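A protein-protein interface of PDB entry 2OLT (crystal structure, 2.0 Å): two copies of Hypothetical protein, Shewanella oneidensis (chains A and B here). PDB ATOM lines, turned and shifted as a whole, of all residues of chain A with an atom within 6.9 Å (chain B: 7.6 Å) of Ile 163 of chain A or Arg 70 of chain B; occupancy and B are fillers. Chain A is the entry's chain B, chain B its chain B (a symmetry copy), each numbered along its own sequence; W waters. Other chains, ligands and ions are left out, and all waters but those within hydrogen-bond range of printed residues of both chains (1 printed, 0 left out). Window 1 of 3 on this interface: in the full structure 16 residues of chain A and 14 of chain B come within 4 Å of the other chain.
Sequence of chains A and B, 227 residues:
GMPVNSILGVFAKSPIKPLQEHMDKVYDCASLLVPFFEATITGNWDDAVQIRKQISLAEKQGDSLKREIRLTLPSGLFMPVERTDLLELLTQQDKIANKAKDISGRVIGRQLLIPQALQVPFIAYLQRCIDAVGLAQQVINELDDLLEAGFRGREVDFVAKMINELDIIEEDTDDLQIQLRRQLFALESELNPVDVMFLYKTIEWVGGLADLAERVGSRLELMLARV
The side-chain amide oxygen (OD1) of Asn 164 of chain A is in hydrogen-bond range of the guanidinium group (NH1) of Arg 67 of chain B, at 3.0 Å. The side-chain carboxylate of Glu 221 of chain A lies within salt-bridge range of the guanidinium group of Arg 70 of chain B (2.7 Å).
The backbone carbonyl oxygen (O) of Ala 160 of chain A lies close to the side-chain amide nitrogen (ND2) of Asn 164 of chain A, at 3.4 Å.
Among the printed residues, pairs that only touch across the chains: Val 156 of chain A with Leu 71 of chain B (3.6 Å), Val 159 of chain A with Leu 71 of chain B (3.9 Å), Ala 160 of chain A with Arg 67 of chain B (3.9 Å), Ala 160 of chain A with Leu 71 of chain B (3.6 Å), Ile 163 of chain A with Arg 67 of chain B (3.3 Å) and Ile 163 of chain A with Arg 70 of chain B (3.4 Å).
Of chain B, only Arg 67 and Arg 70 come within 4 Å of Ile 163 of chain A. Arg 70 of chain B touches just these residues of chain A: Ile 163 and Glu 221. Of the printed residues of chain A, Arg 67 of chain B touches Ala 160 (3.9 Å), Ile 163 (3.3 Å) and Asn 164 (3.0 Å). Printed residues of chain B within 4 Å of Ala 160 of chain A: Arg 67 (3.9 Å) and Leu 71 (3.6 Å). Printed residues of chain A within 4 Å of Leu 71 of chain B: Val 156 (3.6 Å), Val 159 (3.9 Å) and Ala 160 (3.6 Å). Of the printed residues of chain B, Asn 164 of chain A touches Arg 67 (3.0 Å). Of the printed residues of chain B, Val 159 of chain A touches Leu 71. The nearest residue of chain B that does not touch Ile 163 of chain A is Leu 71 of chain B (4.2 Å). The nearest printed residue of chain B that does not touch Ala 160 of chain A is Arg 70 of chain B (6.9 Å).
Hydrophobic or aromatic side chains of chain B that line the printed part of chain A: Leu 71. Of the 16 printed residues of chain A, 6 touch a printed residue of chain B. Hydrophobic or aromatic side chains of chain A that line the printed part of chain B: Val 156, Val 159, Ala 160 and Ile 163. Along chain A the printed residues that touch a printed residue of chain B span positions 156 to 221. Among the printed residues, 8 pairs touch across the chains. Among the printed residues, Asp or Glu carboxylates within 4 Å of a Lys or Arg side-chain nitrogen of the other chain: Glu 221 of chain A with Arg 70 of chain B (2.7 Å).
No position is printed for both chains.
Water W1 lies within hydrogen-bond range of the side-chain carboxylate of Glu 221 of chain A (2.5 Å) and the backbone carbonyl oxygen of Arg 70 of chain B (3.0 Å).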
ATOM      1  N   LEU A 135     -17.641  17.713 -15.606  1.00  0.00           N
ATOM      2  CA  LEU A 135     -16.363  18.268 -16.018  1.00  0.00           C
ATOM      3  C   LEU A 135     -16.544  19.708 -16.518  1.00  0.00           C
ATOM      4  O   LEU A 135     -15.739  20.597 -16.207  1.00  0.00           O
ATOM      5  CB  LEU A 135     -15.704  17.433 -17.094  1.00  0.00           C
ATOM      6  CG  LEU A 135     -14.352  17.967 -17.616  1.00  0.00           C
ATOM      7  CD1 LEU A 135     -13.338  18.092 -16.509  1.00  0.00           C
ATOM      8  CD2 LEU A 135     -13.832  17.047 -18.701  1.00  0.00           C
ATOM      9  N   VAL A 156      -2.477  27.301 -21.606  1.00  0.00           N
ATOM     10  CA  VAL A 156      -2.180  26.088 -22.347  1.00  0.00           C
ATOM     11  C   VAL A 156      -2.283  24.865 -21.432  1.00  0.00           C
ATOM     12  O   VAL A 156      -2.836  23.846 -21.839  1.00  0.00           O
ATOM     13  CB  VAL A 156      -0.809  26.185 -23.049  1.00  0.00           C
ATOM     14  CG1 VAL A 156      -0.423  24.854 -23.699  1.00  0.00           C
ATOM     15  CG2 VAL A 156      -0.845  27.308 -24.098  1.00  0.00           C
ATOM     16  N   PHE A 158      -4.095  24.589 -18.769  1.00  0.00           N
ATOM     17  CA  PHE A 158      -5.511  24.449 -18.446  1.00  0.00           C
ATOM     18  C   PHE A 158      -6.244  23.683 -19.551  1.00  0.00           C
ATOM     19  O   PHE A 158      -7.031  22.784 -19.267  1.00  0.00           O
ATOM     20  CB  PHE A 158      -6.116  25.832 -18.240  1.00  0.00           C
ATOM     21  CG  PHE A 158      -7.566  25.836 -17.825  1.00  0.00           C
ATOM     22  CD1 PHE A 158      -8.570  25.792 -18.770  1.00  0.00           C
ATOM     23  CD2 PHE A 158      -7.917  25.973 -16.488  1.00  0.00           C
ATOM     24  CE1 PHE A 158      -9.893  25.833 -18.405  1.00  0.00           C
ATOM     25  CE2 PHE A 158      -9.243  26.015 -16.115  1.00  0.00           C
ATOM     26  CZ  PHE A 158     -10.238  25.949 -17.086  1.00  0.00           C
ATOM     27  N   VAL A 159      -5.986  24.034 -20.805  1.00  0.00           N
ATOM     28  CA  VAL A 159      -6.597  23.325 -21.936  1.00  0.00           C
ATOM     29  C   VAL A 159      -6.043  21.901 -22.054  1.00  0.00           C
ATOM     30  O   VAL A 159      -6.801  20.973 -22.312  1.00  0.00           O
ATOM     31  CB  VAL A 159      -6.442  24.115 -23.250  1.00  0.00           C
ATOM     32  CG1 VAL A 159      -6.804  23.250 -24.479  1.00  0.00           C
ATOM     33  CG2 VAL A 159      -7.328  25.391 -23.188  1.00  0.00           C
ATOM     34  N   ALA A 160      -4.744  21.709 -21.856  1.00  0.00           N
ATOM     35  CA  ALA A 160      -4.170  20.352 -21.880  1.00  0.00           C
ATOM     36  C   ALA A 160      -4.864  19.462 -20.847  1.00  0.00           C
ATOM     37  O   ALA A 160      -5.191  18.313 -21.138  1.00  0.00           O
ATOM     38  CB  ALA A 160      -2.707  20.381 -21.626  1.00  0.00           C
ATOM     39  N   LYS A 161      -5.112  20.010 -19.657  1.00  0.00           N
ATOM     40  CA  LYS A 161      -5.807  19.276 -18.591  1.00  0.00           C
ATOM     41  C   LYS A 161      -7.256  18.930 -18.921  1.00  0.00           C
ATOM     42  O   LYS A 161      -7.703  17.819 -18.703  1.00  0.00           O
ATOM     43  CB  LYS A 161      -5.793  20.085 -17.299  1.00  0.00           C
ATOM     44  CG  LYS A 161      -6.583  19.443 -16.121  1.00  0.00           C
ATOM     45  CD  LYS A 161      -6.341  20.224 -14.793  1.00  0.00           C
ATOM     46  CE  LYS A 161      -7.119  19.618 -13.603  1.00  0.00           C
ATOM     47  N   MET A 162      -8.015  19.898 -19.406  1.00  0.00           N
ATOM     48  CA  MET A 162      -9.393  19.662 -19.770  1.00  0.00           C
ATOM     49  C   MET A 162      -9.491  18.567 -20.856  1.00  0.00           C
ATOM     50  O   MET A 162     -10.365  17.682 -20.772  1.00  0.00           O
ATOM     51  CB  MET A 162     -10.015  20.968 -20.247  1.00  0.00           C
ATOM     52  CG  MET A 162     -11.472  20.856 -20.631  1.00  0.00           C
ATOM     53  SD  MET A 162     -12.065  22.581 -21.349  1.00  0.00           S
ATOM     54  CE  MET A 162     -11.051  22.517 -23.082  1.00  0.00           C
ATOM     55  N   ILE A 163      -8.608  18.624 -21.855  1.00  0.00           N
ATOM     56  CA  ILE A 163      -8.554  17.613 -22.894  1.00  0.00           C
ATOM     57  C   ILE A 163      -8.239  16.238 -22.280  1.00  0.00           C
ATOM     58  O   ILE A 163      -8.891  15.259 -22.615  1.00  0.00           O
ATOM     59  CB  ILE A 163      -7.484  17.924 -23.954  1.00  0.00           C
ATOM     60  CG1 ILE A 163      -7.830  19.216 -24.707  1.00  0.00           C
ATOM     61  CG2 ILE A 163      -7.376  16.747 -24.952  1.00  0.00           C
ATOM     62  CD1 ILE A 163      -6.731  19.668 -25.695  1.00  0.00           C
ATOM     63  N   ASN A 164      -7.236  16.161 -21.401  1.00  0.00           N
ATOM     64  CA  ASN A 164      -6.909  14.900 -20.732  1.00  0.00           C
ATOM     65  C   ASN A 164      -8.115  14.328 -20.005  1.00  0.00           C
ATOM     66  O   ASN A 164      -8.445  13.163 -20.169  1.00  0.00           O
ATOM     67  CB  ASN A 164      -5.761  15.085 -19.732  1.00  0.00           C
ATOM     68  CG  ASN A 164      -4.407  15.218 -20.413  1.00  0.00           C
ATOM     69  OD1 ASN A 164      -4.254  14.793 -21.561  1.00  0.00           O
ATOM     70  ND2 ASN A 164      -3.400  15.787 -19.703  1.00  0.00           N
ATOM     71  N   GLU A 165      -8.798  15.161 -19.230  1.00  0.00           N
ATOM     72  CA  GLU A 165      -9.940  14.697 -18.440  1.00  0.00           C
ATOM     73  C   GLU A 165     -11.106  14.281 -19.318  1.00  0.00           C
ATOM     74  O   GLU A 165     -11.763  13.287 -19.040  1.00  0.00           O
ATOM     75  CB  GLU A 165     -10.302  15.685 -17.314  1.00  0.00           C
ATOM     76  CG  GLU A 165      -9.131  15.792 -16.264  1.00  0.00           C
ATOM     77  CD  GLU A 165      -9.401  16.676 -15.030  1.00  0.00           C
ATOM     78  OE1 GLU A 165     -10.301  17.548 -15.060  1.00  0.00           O
ATOM     79  OE2 GLU A 165      -8.671  16.510 -14.012  1.00  0.00           O
ATOM     80  N   LEU A 166     -11.334  15.004 -20.406  1.00  0.00           N
ATOM     81  CA  LEU A 166     -12.409  14.657 -21.300  1.00  0.00           C
ATOM     82  C   LEU A 166     -12.131  13.366 -22.057  1.00  0.00           C
ATOM     83  O   LEU A 166     -13.064  12.576 -22.236  1.00  0.00           O
ATOM     84  CB  LEU A 166     -12.681  15.772 -22.281  1.00  0.00           C
ATOM     85  CG  LEU A 166     -13.886  15.531 -23.174  1.00  0.00           C
ATOM     86  CD1 LEU A 166     -15.123  15.243 -22.322  1.00  0.00           C
ATOM     87  CD2 LEU A 166     -14.074  16.754 -24.065  1.00  0.00           C
ATOM     88  N   ASP A 167     -10.892  13.164 -22.519  1.00  0.00           N
ATOM     89  CA  ASP A 167     -10.509  11.927 -23.204  1.00  0.00           C
ATOM     90  C   ASP A 167     -10.846  10.700 -22.321  1.00  0.00           C
ATOM     91  O   ASP A 167     -11.289   9.670 -22.824  1.00  0.00           O
ATOM     92  CB  ASP A 167      -8.996  11.885 -23.533  1.00  0.00           C
ATOM     93  CG  ASP A 167      -8.591  12.770 -24.730  1.00  0.00           C
ATOM     94  OD1 ASP A 167      -9.477  13.319 -25.428  1.00  0.00           O
ATOM     95  OD2 ASP A 167      -7.353  12.914 -24.965  1.00  0.00           O
ATOM     96  N   ILE A 168     -10.569  10.807 -21.024  1.00  0.00           N
ATOM     97  CA  ILE A 168     -10.872   9.738 -20.070  1.00  0.00           C
ATOM     98  C   ILE A 168     -12.382   9.483 -20.014  1.00  0.00           C
ATOM     99  O   ILE A 168     -12.838   8.343 -20.109  1.00  0.00           O
ATOM    100  CB  ILE A 168     -10.376  10.084 -18.659  1.00  0.00           C
ATOM    101  CG1 ILE A 168      -8.841  10.076 -18.599  1.00  0.00           C
ATOM    102  CG2 ILE A 168     -10.921   9.085 -17.642  1.00  0.00           C
ATOM    103  N   GLY A 217     -17.011  23.250 -23.080  1.00  0.00           N
ATOM    104  CA  GLY A 217     -15.535  23.301 -23.011  1.00  0.00           C
ATOM    105  C   GLY A 217     -14.912  23.987 -24.214  1.00  0.00           C
ATOM    106  O   GLY A 217     -13.935  24.722 -24.074  1.00  0.00           O
ATOM    107  N   SER A 218     -15.457  23.726 -25.403  1.00  0.00           N
ATOM    108  CA  SER A 218     -14.973  24.337 -26.644  1.00  0.00           C
ATOM    109  C   SER A 218     -15.091  25.857 -26.629  1.00  0.00           C
ATOM    110  O   SER A 218     -14.219  26.560 -27.078  1.00  0.00           O
ATOM    111  CB  SER A 218     -15.764  23.857 -27.885  1.00  0.00           C
ATOM    112  OG  SER A 218     -15.445  22.540 -28.169  1.00  0.00           O
ATOM    113  N   GLU A 221     -12.496  27.231 -24.414  1.00  0.00           N
ATOM    114  CA  GLU A 221     -11.237  27.183 -25.122  1.00  0.00           C
ATOM    115  C   GLU A 221     -11.110  28.332 -26.110  1.00  0.00           C
ATOM    116  O   GLU A 221     -10.041  28.924 -26.242  1.00  0.00           O
ATOM    117  CB  GLU A 221     -11.111  25.819 -25.786  1.00  0.00           C
ATOM    118  CG  GLU A 221      -9.831  25.611 -26.452  1.00  0.00           C
ATOM    119  CD  GLU A 221      -9.686  24.224 -27.034  1.00  0.00           C
ATOM    120  OE1 GLU A 221     -10.509  23.356 -26.697  1.00  0.00           O
ATOM    121  OE2 GLU A 221      -8.712  24.017 -27.796  1.00  0.00           O
ATOM    122  N   ASP B  63      -6.976  13.035 -34.218  1.00  0.00           N
ATOM    123  CA  ASP B  63      -7.144  13.574 -32.886  1.00  0.00           C
ATOM    124  C   ASP B  63      -5.788  14.082 -32.313  1.00  0.00           C
ATOM    125  O   ASP B  63      -5.741  15.082 -31.600  1.00  0.00           O
ATOM    126  CB  ASP B  63      -7.762  12.512 -31.966  1.00  0.00           C
ATOM    127  CG  ASP B  63      -8.174  13.069 -30.609  1.00  0.00           C
ATOM    128  OD1 ASP B  63      -8.991  14.035 -30.540  1.00  0.00           O
ATOM    129  OD2 ASP B  63      -7.684  12.533 -29.605  1.00  0.00           O
ATOM    130  N   SER B  64      -4.688  13.385 -32.611  1.00  0.00           N
ATOM    131  CA  SER B  64      -3.390  13.818 -32.144  1.00  0.00           C
ATOM    132  C   SER B  64      -2.974  15.119 -32.762  1.00  0.00           C
ATOM    133  O   SER B  64      -2.439  15.977 -32.073  1.00  0.00           O
ATOM    134  CB  SER B  64      -2.299  12.807 -32.436  1.00  0.00           C
ATOM    135  OG  SER B  64      -2.383  11.733 -31.526  1.00  0.00           O
ATOM    136  N   LEU B  65      -3.166  15.239 -34.070  1.00  0.00           N
ATOM    137  CA  LEU B  65      -2.849  16.460 -34.773  1.00  0.00           C
ATOM    138  C   LEU B  65      -3.695  17.575 -34.184  1.00  0.00           C
ATOM    139  O   LEU B  65      -3.212  18.675 -34.015  1.00  0.00           O
ATOM    140  CB  LEU B  65      -3.128  16.350 -36.274  1.00  0.00           C
ATOM    141  CG  LEU B  65      -2.278  15.356 -37.063  1.00  0.00           C
ATOM    142  CD1 LEU B  65      -2.686  15.299 -38.531  1.00  0.00           C
ATOM    143  CD2 LEU B  65      -0.841  15.756 -36.957  1.00  0.00           C
ATOM    144  N   LYS B  66      -4.956  17.272 -33.895  1.00  0.00           N
ATOM    145  CA  LYS B  66      -5.887  18.224 -33.289  1.00  0.00           C
ATOM    146  C   LYS B  66      -5.386  18.722 -31.947  1.00  0.00           C
ATOM    147  O   LYS B  66      -5.422  19.921 -31.665  1.00  0.00           O
ATOM    148  CB  LYS B  66      -7.255  17.572 -33.075  1.00  0.00           C
ATOM    149  CG  LYS B  66      -8.315  18.529 -32.566  1.00  0.00           C
ATOM    150  CD  LYS B  66      -9.689  17.907 -32.416  1.00  0.00           C
ATOM    151  CE  LYS B  66      -9.738  16.952 -31.271  1.00  0.00           C
ATOM    152  NZ  LYS B  66     -11.146  16.546 -30.967  1.00  0.00           N
ATOM    153  N   ARG B  67      -4.947  17.780 -31.108  1.00  0.00           N
ATOM    154  CA  ARG B  67      -4.451  18.106 -29.792  1.00  0.00           C
ATOM    155  C   ARG B  67      -3.255  19.045 -29.922  1.00  0.00           C
ATOM    156  O   ARG B  67      -3.209  20.082 -29.265  1.00  0.00           O
ATOM    157  CB  ARG B  67      -4.071  16.849 -29.003  1.00  0.00           C
ATOM    158  CG  ARG B  67      -3.607  17.153 -27.591  1.00  0.00           C
ATOM    159  CD  ARG B  67      -3.012  15.943 -26.875  1.00  0.00           C
ATOM    160  NE  ARG B  67      -2.401  16.398 -25.628  1.00  0.00           N
ATOM    161  CZ  ARG B  67      -3.004  16.444 -24.439  1.00  0.00           C
ATOM    162  NH1 ARG B  67      -4.258  16.015 -24.288  1.00  0.00           N
ATOM    163  NH2 ARG B  67      -2.336  16.896 -23.385  1.00  0.00           N
ATOM    164  N   GLU B  68      -2.315  18.715 -30.800  1.00  0.00           N
ATOM    165  CA  GLU B  68      -1.114  19.542 -30.959  1.00  0.00           C
ATOM    166  C   GLU B  68      -1.469  20.957 -31.415  1.00  0.00           C
ATOM    167  O   GLU B  68      -0.925  21.931 -30.884  1.00  0.00           O
ATOM    168  CB  GLU B  68      -0.101  18.905 -31.919  1.00  0.00           C
ATOM    169  N   ILE B  69      -2.384  21.078 -32.374  1.00  0.00           N
ATOM    170  CA  ILE B  69      -2.793  22.405 -32.828  1.00  0.00           C
ATOM    171  C   ILE B  69      -3.424  23.190 -31.685  1.00  0.00           C
ATOM    172  O   ILE B  69      -3.120  24.350 -31.511  1.00  0.00           O
ATOM    173  CB  ILE B  69      -3.765  22.343 -34.013  1.00  0.00           C
ATOM    174  CG1 ILE B  69      -3.071  21.773 -35.249  1.00  0.00           C
ATOM    175  CG2 ILE B  69      -4.348  23.728 -34.330  1.00  0.00           C
ATOM    176  CD1 ILE B  69      -4.047  21.190 -36.279  1.00  0.00           C
ATOM    177  N   ARG B  70      -4.290  22.552 -30.905  1.00  0.00           N
ATOM    178  CA  ARG B  70      -4.970  23.221 -29.782  1.00  0.00           C
ATOM    179  C   ARG B  70      -4.030  23.717 -28.711  1.00  0.00           C
ATOM    180  O   ARG B  70      -4.291  24.749 -28.072  1.00  0.00           O
ATOM    181  CB  ARG B  70      -6.005  22.292 -29.163  1.00  0.00           C
ATOM    182  CG  ARG B  70      -7.183  22.090 -30.064  1.00  0.00           C
ATOM    183  CD  ARG B  70      -8.057  20.934 -29.633  1.00  0.00           C
ATOM    184  NE  ARG B  70      -8.817  21.213 -28.431  1.00  0.00           N
ATOM    185  CZ  ARG B  70      -9.498  20.289 -27.763  1.00  0.00           C
ATOM    186  NH1 ARG B  70      -9.451  19.012 -28.113  1.00  0.00           N
ATOM    187  NH2 ARG B  70     -10.188  20.632 -26.698  1.00  0.00           N
ATOM    188  N   LEU B  71      -2.941  22.983 -28.509  1.00  0.00           N
ATOM    189  CA  LEU B  71      -1.965  23.341 -27.505  1.00  0.00           C
ATOM    190  C   LEU B  71      -0.848  24.245 -28.044  1.00  0.00           C
ATOM    191  O   LEU B  71       0.011  24.693 -27.283  1.00  0.00           O
ATOM    192  CB  LEU B  71      -1.393  22.083 -26.847  1.00  0.00           C
ATOM    193  CG  LEU B  71      -2.444  21.184 -26.170  1.00  0.00           C
ATOM    194  CD1 LEU B  71      -1.807  19.931 -25.583  1.00  0.00           C
ATOM    195  CD2 LEU B  71      -3.215  21.956 -25.096  1.00  0.00           C
ATOM    196  N   THR B  72      -0.893  24.547 -29.339  1.00  0.00           N
ATOM    197  CA  THR B  72       0.105  25.400 -29.991  1.00  0.00           C
ATOM    198  C   THR B  72      -0.437  26.767 -30.448  1.00  0.00           C
ATOM    199  O   THR B  72       0.131  27.810 -30.129  1.00  0.00           O
ATOM    200  CB  THR B  72       0.664  24.684 -31.223  1.00  0.00           C
ATOM    201  OG1 THR B  72       1.416  23.548 -30.800  1.00  0.00           O
ATOM    202  CG2 THR B  72       1.578  25.602 -31.999  1.00  0.00           C
ATOM    203  N   LEU B  73      -1.519  26.738 -31.219  1.00  0.00           N
ATOM    204  CA  LEU B  73      -2.170  27.929 -31.780  1.00  0.00           C
ATOM    205  C   LEU B  73      -2.069  29.075 -30.770  1.00  0.00           C
ATOM    206  O   LEU B  73      -1.412  30.077 -31.072  1.00  0.00           O
ATOM    207  CB  LEU B  73      -3.631  27.621 -32.176  1.00  0.00           C
ATOM    208  CG  LEU B  73      -4.233  28.212 -33.459  1.00  0.00           C
ATOM    209  N   PRO B  74      -2.667  28.924 -29.550  1.00  0.00           N
ATOM    210  CA  PRO B  74      -2.562  29.989 -28.513  1.00  0.00           C
ATOM    211  C   PRO B  74      -1.189  30.663 -28.471  1.00  0.00           C
ATOM    212  O   PRO B  74      -1.110  31.888 -28.377  1.00  0.00           O
ATOM    213  CB  PRO B  74      -2.830  29.239 -27.182  1.00  0.00           C
ATOM    214  CG  PRO B  74      -3.116  27.771 -27.556  1.00  0.00           C
ATOM    215  CD  PRO B  74      -3.469  27.791 -29.042  1.00  0.00           C
ATOM    216  N   SER B  75      -0.118  29.867 -28.520  1.00  0.00           N
ATOM    217  CA  SER B  75       1.253  30.406 -28.594  1.00  0.00           C
ATOM    218  C   SER B  75       1.772  31.232 -29.757  1.00  0.00           C
ATOM    219  O   SER B  75       2.938  31.642 -29.812  1.00  0.00           O
ATOM    220  CB  SER B  75       2.293  29.722 -27.681  1.00  0.00           C
ATOM    221  N   LEU B  87      -9.426  27.350 -34.762  1.00  0.00           N
ATOM    222  CA  LEU B  87      -9.953  26.378 -33.816  1.00  0.00           C
ATOM    223  C   LEU B  87     -11.328  25.920 -34.260  1.00  0.00           C
ATOM    224  O   LEU B  87     -11.627  24.741 -34.190  1.00  0.00           O
ATOM    225  CB  LEU B  87     -10.021  26.941 -32.387  1.00  0.00           C
ATOM    226  CG  LEU B  87      -8.693  27.155 -31.659  1.00  0.00           C
ATOM    227  CD1 LEU B  87      -8.930  27.751 -30.272  1.00  0.00           C
ATOM    228  CD2 LEU B  87      -7.915  25.866 -31.550  1.00  0.00           C
ATOM    229  N   LEU B  90     -10.983  23.557 -37.120  1.00  0.00           N
ATOM    230  CA  LEU B  90     -10.521  22.290 -36.603  1.00  0.00           C
ATOM    231  C   LEU B  90     -11.626  21.464 -35.983  1.00  0.00           C
ATOM    232  O   LEU B  90     -11.687  20.231 -36.165  1.00  0.00           O
ATOM    233  CB  LEU B  90      -9.431  22.570 -35.571  1.00  0.00           C
ATOM    234  CG  LEU B  90      -8.651  21.393 -35.042  1.00  0.00           C
ATOM    235  CD1 LEU B  90      -7.920  20.619 -36.161  1.00  0.00           C
ATOM    236  CD2 LEU B  90      -7.680  21.943 -34.008  1.00  0.00           C
ATOM    237  N   THR B  91     -12.510  22.121 -35.237  1.00  0.00           N
ATOM    238  CA  THR B  91     -13.627  21.431 -34.621  1.00  0.00           C
ATOM    239  C   THR B  91     -14.531  20.825 -35.674  1.00  0.00           C
ATOM    240  O   THR B  91     -14.979  19.680 -35.502  1.00  0.00           O
ATOM    241  CB  THR B  91     -14.403  22.362 -33.684  1.00  0.00           C
ATOM    242  OG1 THR B  91     -13.498  22.880 -32.732  1.00  0.00           O
ATOM    243  CG2 THR B  91     -15.490  21.641 -32.943  1.00  0.00           C
ATOM    244  N   ASP B  94     -12.735  17.830 -37.453  1.00  0.00           N
ATOM    245  CA  ASP B  94     -12.662  16.672 -36.584  1.00  0.00           C
ATOM    246  C   ASP B  94     -13.946  15.847 -36.565  1.00  0.00           C
ATOM    247  O   ASP B  94     -13.884  14.618 -36.464  1.00  0.00           O
ATOM    248  CB  ASP B  94     -12.323  17.129 -35.165  1.00  0.00           C
ATOM    249  CG  ASP B  94     -12.452  16.012 -34.095  1.00  0.00           C
ATOM    250  OD1 ASP B  94     -11.576  15.150 -34.030  1.00  0.00           O
ATOM    251  OD2 ASP B  94     -13.397  16.069 -33.231  1.00  0.00           O
HETATM  252  O   HOH W   1      -7.045  25.885 -27.761  1.00  0.00           O
